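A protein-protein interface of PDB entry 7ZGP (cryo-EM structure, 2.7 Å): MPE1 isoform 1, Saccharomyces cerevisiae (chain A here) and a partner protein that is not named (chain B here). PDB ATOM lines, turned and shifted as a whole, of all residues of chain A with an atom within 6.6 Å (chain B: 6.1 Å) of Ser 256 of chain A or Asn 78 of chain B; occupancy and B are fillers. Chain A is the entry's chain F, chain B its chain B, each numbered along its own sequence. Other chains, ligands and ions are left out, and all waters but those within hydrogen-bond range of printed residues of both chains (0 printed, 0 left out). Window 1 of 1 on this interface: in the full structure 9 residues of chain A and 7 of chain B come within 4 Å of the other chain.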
ATOM      1  N   PHE A 218     -21.916  27.819  16.992  1.00  0.00           N
ATOM      2  CA  PHE A 218     -20.610  27.803  16.283  1.00  0.00           C
ATOM      3  C   PHE A 218     -19.523  28.101  17.319  1.00  0.00           C
ATOM      4  O   PHE A 218     -18.386  28.406  16.916  1.00  0.00           O
ATOM      5  CB  PHE A 218     -20.627  28.814  15.135  1.00  0.00           C
ATOM      6  CG  PHE A 218     -21.839  28.719  14.243  1.00  0.00           C
ATOM      7  CD1 PHE A 218     -21.916  27.758  13.248  1.00  0.00           C
ATOM      8  CD2 PHE A 218     -22.906  29.587  14.403  1.00  0.00           C
ATOM      9  CE1 PHE A 218     -23.032  27.670  12.432  1.00  0.00           C
ATOM     10  CE2 PHE A 218     -24.021  29.499  13.585  1.00  0.00           C
ATOM     11  CZ  PHE A 218     -24.083  28.541  12.602  1.00  0.00           C
ATOM     12  N   ASP A 253     -18.760  26.964  10.054  1.00  0.00           N
ATOM     13  CA  ASP A 253     -19.905  26.032   9.870  1.00  0.00           C
ATOM     14  C   ASP A 253     -19.519  25.079   8.735  1.00  0.00           C
ATOM     15  O   ASP A 253     -19.939  25.321   7.588  1.00  0.00           O
ATOM     16  CB  ASP A 253     -21.240  26.763   9.677  1.00  0.00           C
ATOM     17  CG  ASP A 253     -21.344  27.595   8.412  1.00  0.00           C
ATOM     18  OD1 ASP A 253     -20.302  27.840   7.788  1.00  0.00           O
ATOM     19  OD2 ASP A 253     -22.474  27.986   8.062  1.00  0.00           O
ATOM     20  N   LYS A 254     -18.732  24.045   9.045  1.00  0.00           N
ATOM     21  CA  LYS A 254     -18.242  23.115   7.992  1.00  0.00           C
ATOM     22  C   LYS A 254     -19.418  22.297   7.456  1.00  0.00           C
ATOM     23  O   LYS A 254     -19.266  21.070   7.319  1.00  0.00           O
ATOM     24  CB  LYS A 254     -17.139  22.214   8.560  1.00  0.00           C
ATOM     25  N   GLN A 255     -20.548  22.950   7.188  1.00  0.00           N
ATOM     26  CA  GLN A 255     -21.716  22.261   6.585  1.00  0.00           C
ATOM     27  C   GLN A 255     -22.155  23.103   5.388  1.00  0.00           C
ATOM     28  O   GLN A 255     -22.373  22.529   4.309  1.00  0.00           O
ATOM     29  CB  GLN A 255     -22.842  22.112   7.607  1.00  0.00           C
ATOM     30  CG  GLN A 255     -24.107  21.497   7.027  1.00  0.00           C
ATOM     31  CD  GLN A 255     -25.203  21.371   8.055  1.00  0.00           C
ATOM     32  OE1 GLN A 255     -25.046  21.762   9.210  1.00  0.00           O
ATOM     33  NE2 GLN A 255     -26.332  20.818   7.640  1.00  0.00           N
ATOM     34  N   SER A 256     -22.252  24.420   5.580  1.00  0.00           N
ATOM     35  CA  SER A 256     -22.600  25.327   4.458  1.00  0.00           C
ATOM     36  C   SER A 256     -21.497  25.254   3.401  1.00  0.00           C
ATOM     37  O   SER A 256     -21.828  25.208   2.203  1.00  0.00           O
ATOM     38  CB  SER A 256     -22.801  26.734   4.947  1.00  0.00           C
ATOM     39  OG  SER A 256     -23.829  26.785   5.925  1.00  0.00           O
ATOM     40  N   TRP A 257     -20.236  25.230   3.838  1.00  0.00           N
ATOM     41  CA  TRP A 257     -19.101  25.120   2.885  1.00  0.00           C
ATOM     42  C   TRP A 257     -19.188  23.778   2.157  1.00  0.00           C
ATOM     43  O   TRP A 257     -18.954  23.755   0.936  1.00  0.00           O
ATOM     44  CB  TRP A 257     -17.760  25.284   3.610  1.00  0.00           C
ATOM     45  CG  TRP A 257     -16.592  25.401   2.682  1.00  0.00           C
ATOM     46  CD1 TRP A 257     -15.601  24.484   2.484  1.00  0.00           C
ATOM     47  CD2 TRP A 257     -16.298  26.504   1.807  1.00  0.00           C
ATOM     48  NE1 TRP A 257     -14.708  24.943   1.554  1.00  0.00           N
ATOM     49  CE2 TRP A 257     -15.109  26.179   1.120  1.00  0.00           C
ATOM     50  CE3 TRP A 257     -16.917  27.729   1.540  1.00  0.00           C
ATOM     51  CZ2 TRP A 257     -14.533  27.038   0.185  1.00  0.00           C
ATOM     52  CZ3 TRP A 257     -16.348  28.577   0.617  1.00  0.00           C
ATOM     53  CH2 TRP A 257     -15.171  28.233  -0.049  1.00  0.00           C
ATOM     54  N   GLU A 258     -19.520  22.709   2.886  1.00  0.00           N
ATOM     55  CA  GLU A 258     -19.640  21.362   2.270  1.00  0.00           C
ATOM     56  C   GLU A 258     -20.782  21.373   1.251  1.00  0.00           C
ATOM     57  O   GLU A 258     -20.577  20.858   0.138  1.00  0.00           O
ATOM     58  CB  GLU A 258     -19.870  20.308   3.353  1.00  0.00           C
ATOM     59  CG  GLU A 258     -18.705  20.178   4.315  1.00  0.00           C
ATOM     60  CD  GLU A 258     -18.842  19.050   5.322  1.00  0.00           C
ATOM     61  OE1 GLU A 258     -19.903  18.395   5.331  1.00  0.00           O
ATOM     62  OE2 GLU A 258     -17.888  18.830   6.094  1.00  0.00           O
ATOM     63  N   ASP A 259     -21.932  21.943   1.618  1.00  0.00           N
ATOM     64  CA  ASP A 259     -23.071  22.049   0.669  1.00  0.00           C
ATOM     65  C   ASP A 259     -22.590  22.790  -0.579  1.00  0.00           C
ATOM     66  O   ASP A 259     -22.916  22.343  -1.692  1.00  0.00           O
ATOM     67  CB  ASP A 259     -24.271  22.733   1.325  1.00  0.00           C
ATOM     68  CG  ASP A 259     -24.743  22.029   2.585  1.00  0.00           C
ATOM     69  OD1 ASP A 259     -24.233  20.925   2.864  1.00  0.00           O
ATOM     70  OD2 ASP A 259     -25.611  22.591   3.281  1.00  0.00           O
ATOM     71  N   TYR A 260     -21.840  23.876  -0.392  1.00  0.00           N
ATOM     72  CA  TYR A 260     -21.282  24.643  -1.531  1.00  0.00           C
ATOM     73  C   TYR A 260     -20.428  23.693  -2.369  1.00  0.00           C
ATOM     74  O   TYR A 260     -20.499  23.754  -3.612  1.00  0.00           O
ATOM     75  CB  TYR A 260     -20.466  25.833  -1.025  1.00  0.00           C
ATOM     76  CG  TYR A 260     -19.500  26.409  -2.029  1.00  0.00           C
ATOM     77  CD1 TYR A 260     -19.951  27.006  -3.194  1.00  0.00           C
ATOM     78  CD2 TYR A 260     -18.134  26.367  -1.809  1.00  0.00           C
ATOM     79  CE1 TYR A 260     -19.070  27.542  -4.118  1.00  0.00           C
ATOM     80  CE2 TYR A 260     -17.239  26.898  -2.722  1.00  0.00           C
ATOM     81  CZ  TYR A 260     -17.709  27.489  -3.881  1.00  0.00           C
ATOM     82  OH  TYR A 260     -16.834  28.014  -4.787  1.00  0.00           O
ATOM     83  N   GLN A 261     -19.653  22.837  -1.699  1.00  0.00           N
ATOM     84  CA  GLN A 261     -18.814  21.848  -2.418  1.00  0.00           C
ATOM     85  C   GLN A 261     -19.741  20.874  -3.150  1.00  0.00           C
ATOM     86  O   GLN A 261     -19.516  20.637  -4.354  1.00  0.00           O
ATOM     87  CB  GLN A 261     -17.893  21.120  -1.438  1.00  0.00           C
ATOM     88  CG  GLN A 261     -17.006  22.055  -0.633  1.00  0.00           C
ATOM     89  CD  GLN A 261     -16.169  22.946  -1.517  1.00  0.00           C
ATOM     90  OE1 GLN A 261     -15.759  22.564  -2.611  1.00  0.00           O
ATOM     91  NE2 GLN A 261     -15.900  24.149  -1.039  1.00  0.00           N
ATOM     92  N   ILE B  60     -37.182  22.373   9.211  1.00  0.00           N
ATOM     93  CA  ILE B  60     -37.167  23.811   9.450  1.00  0.00           C
ATOM     94  C   ILE B  60     -38.572  24.398   9.450  1.00  0.00           C
ATOM     95  O   ILE B  60     -38.820  25.410  10.115  1.00  0.00           O
ATOM     96  CB  ILE B  60     -36.267  24.501   8.400  1.00  0.00           C
ATOM     97  CG1 ILE B  60     -36.177  26.008   8.645  1.00  0.00           C
ATOM     98  CG2 ILE B  60     -36.762  24.214   6.994  1.00  0.00           C
ATOM     99  CD1 ILE B  60     -35.423  26.379   9.891  1.00  0.00           C
ATOM    100  N   CYS B  75     -29.965  35.121   8.861  1.00  0.00           N
ATOM    101  CA  CYS B  75     -30.009  33.909   9.671  1.00  0.00           C
ATOM    102  C   CYS B  75     -28.742  33.101   9.422  1.00  0.00           C
ATOM    103  O   CYS B  75     -28.489  32.665   8.294  1.00  0.00           O
ATOM    104  CB  CYS B  75     -31.247  33.077   9.345  1.00  0.00           C
ATOM    105  SG  CYS B  75     -31.399  31.566  10.324  1.00  0.00           S
ATOM    106  N   LYS B  76     -27.951  32.899  10.475  1.00  0.00           N
ATOM    107  CA  LYS B  76     -26.692  32.178  10.350  1.00  0.00           C
ATOM    108  C   LYS B  76     -26.853  30.667  10.421  1.00  0.00           C
ATOM    109  O   LYS B  76     -25.892  29.946  10.134  1.00  0.00           O
ATOM    110  CB  LYS B  76     -25.715  32.636  11.436  1.00  0.00           C
ATOM    111  CG  LYS B  76     -25.225  34.062  11.266  1.00  0.00           C
ATOM    112  CD  LYS B  76     -24.386  34.498  12.454  1.00  0.00           C
ATOM    113  CE  LYS B  76     -24.300  36.009  12.544  1.00  0.00           C
ATOM    114  NZ  LYS B  76     -23.608  36.589  11.366  1.00  0.00           N
ATOM    115  N   LYS B  77     -28.031  30.168  10.791  1.00  0.00           N
ATOM    116  CA  LYS B  77     -28.234  28.738  10.955  1.00  0.00           C
ATOM    117  C   LYS B  77     -28.836  28.062   9.731  1.00  0.00           C
ATOM    118  O   LYS B  77     -28.711  26.840   9.600  1.00  0.00           O
ATOM    119  CB  LYS B  77     -29.126  28.472  12.172  1.00  0.00           C
ATOM    120  CG  LYS B  77     -28.545  28.987  13.474  1.00  0.00           C
ATOM    121  CD  LYS B  77     -29.511  28.793  14.624  1.00  0.00           C
ATOM    122  CE  LYS B  77     -28.992  29.447  15.892  1.00  0.00           C
ATOM    123  NZ  LYS B  77     -30.041  29.525  16.942  1.00  0.00           N
ATOM    124  N   ASN B  78     -29.477  28.820   8.846  1.00  0.00           N
ATOM    125  CA  ASN B  78     -30.033  28.312   7.582  1.00  0.00           C
ATOM    126  C   ASN B  78     -31.057  27.231   7.922  1.00  0.00           C
ATOM    127  O   ASN B  78     -31.897  27.452   8.810  1.00  0.00           O
ATOM    128  CB  ASN B  78     -28.892  27.878   6.671  1.00  0.00           C
ATOM    129  CG  ASN B  78     -27.857  28.968   6.477  1.00  0.00           C
ATOM    130  OD1 ASN B  78     -28.164  30.048   5.976  1.00  0.00           O
ATOM    131  ND2 ASN B  78     -26.624  28.689   6.879  1.00  0.00           N
ATOM    132  N   ASP B  79     -31.034  26.070   7.265  1.00  0.00           N
ATOM    133  CA  ASP B  79     -32.028  25.032   7.507  1.00  0.00           C
ATOM    134  C   ASP B  79     -31.891  24.382   8.877  1.00  0.00           C
ATOM    135  O   ASP B  79     -32.813  23.676   9.301  1.00  0.00           O
ATOM    136  CB  ASP B  79     -31.937  23.960   6.420  1.00  0.00           C
ATOM    137  CG  ASP B  79     -32.065  24.537   5.024  1.00  0.00           C
ATOM    138  OD1 ASP B  79     -33.171  24.994   4.668  1.00  0.00           O
ATOM    139  OD2 ASP B  79     -31.059  24.532   4.285  1.00  0.00           O
ATOM    140  N   GLN B  80     -30.779  24.597   9.575  1.00  0.00           N
ATOM    141  CA  GLN B  80     -30.593  24.044  10.908  1.00  0.00           C
ATOM    142  C   GLN B  80     -31.183  24.927  11.999  1.00  0.00           C
ATOM    143  O   GLN B  80     -31.077  24.578  13.180  1.00  0.00           O
ATOM    144  CB  GLN B  80     -29.106  23.812  11.180  1.00  0.00           C
ATOM    145  CG  GLN B  80     -28.300  23.404   9.959  1.00  0.00           C
ATOM    146  CD  GLN B  80     -28.874  22.190   9.257  1.00  0.00           C
ATOM    147  OE1 GLN B  80     -29.115  21.156   9.878  1.00  0.00           O
ATOM    148  NE2 GLN B  80     -29.093  22.309   7.953  1.00  0.00           N
ATOM    149  N   CYS B  81     -31.789  26.054  11.635  1.00  0.00           N
ATOM    150  CA  CYS B  81     -32.371  26.953  12.620  1.00  0.00           C
ATOM    151  C   CYS B  81     -33.532  26.281  13.342  1.00  0.00           C
ATOM    152  O   CYS B  81     -34.269  25.475  12.770  1.00  0.00           O
ATOM    153  CB  CYS B  81     -32.845  28.240  11.943  1.00  0.00           C
ATOM    154  SG  CYS B  81     -33.249  29.590  13.069  1.00  0.00           S
ATOM    155  N   TYR B  83     -36.015  28.004  14.536  1.00  0.00           N
ATOM    156  CA  TYR B  83     -37.160  28.875  14.342  1.00  0.00           C
ATOM    157  C   TYR B  83     -37.631  28.803  12.896  1.00  0.00           C
ATOM    158  O   TYR B  83     -36.888  28.409  11.994  1.00  0.00           O
ATOM    159  CB  TYR B  83     -36.821  30.317  14.730  1.00  0.00           C
ATOM    160  CG  TYR B  83     -36.776  30.529  16.224  1.00  0.00           C
ATOM    161  CD1 TYR B  83     -35.671  30.140  16.968  1.00  0.00           C
ATOM    162  CD2 TYR B  83     -37.842  31.110  16.892  1.00  0.00           C
ATOM    163  CE1 TYR B  83     -35.630  30.324  18.335  1.00  0.00           C
ATOM    164  CE2 TYR B  83     -37.809  31.301  18.259  1.00  0.00           C
ATOM    165  CZ  TYR B  83     -36.702  30.906  18.974  1.00  0.00           C
ATOM    166  OH  TYR B  83     -36.665  31.095  20.335  1.00  0.00           O
ATOM    167  N   HIS B  85     -38.545  29.356   9.208  1.00  0.00           N
ATOM    168  CA  HIS B  85     -38.056  30.118   8.061  1.00  0.00           C
ATOM    169  C   HIS B  85     -39.129  30.270   6.993  1.00  0.00           C
ATOM    170  O   HIS B  85     -38.842  30.248   5.795  1.00  0.00           O
ATOM    171  CB  HIS B  85     -36.804  29.471   7.481  1.00  0.00           C
ATOM    172  CG  HIS B  85     -35.544  29.871   8.181  1.00  0.00           C
ATOM    173  ND1 HIS B  85     -34.302  29.775   7.592  1.00  0.00           N
ATOM    174  CD2 HIS B  85     -35.335  30.372   9.421  1.00  0.00           C
ATOM    175  CE1 HIS B  85     -33.382  30.199   8.440  1.00  0.00           C
ATOM    176  NE2 HIS B  85     -33.982  30.566   9.557  1.00  0.00           N
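Of the printed residues of chain B, Phe 218 of chain A touches Lys 76 (3.4 Å).
Of the printed residues of chain B, Gln 255 of chain A touches Gln 80 (3.2 Å).
Gln 261 of chain A touches none of the printed residues of chain B.
SG of Cys 75 of chain B sits close to N of Asn 78 of chain B (3.7 Å).
The side-chain carboxylate of Asp 253 of chain A is in hydrogen-bond range of the side-chain hydroxyl of Ser 256 of chain A (2.8 Å).
The side-chain amide nitrogen (NE2) of Gln 80 of chain B sits close to the side-chain amide nitrogen (NE2) of Gln 255 of chain A.
Of the 10 printed residues of chain A, 3 touch a printed residue of chain B.
Printed residues of chain A that touch a printed residue of chain B: Phe 218, Gln 255 and Ser 256.
Hydrophobic or aromatic side chains of chain A within 4 Å of the printed part of chain B: Phe 218.
Along chain A the printed residues that touch a printed residue of chain B span positions 218 to 256.
Of the 10 printed residues of chain B, 3 touch a printed residue of chain A.
Printed residues of chain B that touch a printed residue of chain A: Lys 76, Asn 78 and Gln 80.
Among the printed residues, 3 pairs touch across the chains.
Among the printed residues, no Asp or Glu carboxylate lies within 4 Å of a Lys or Arg side-chain nitrogen of the other chain.
Among the printed residues, pairs that only touch across the chains: Phe 218 of chain A with Lys 76 of chain B (3.4 Å) and Ser 256 of chain A with Asn 78 of chain B (3.5 Å).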
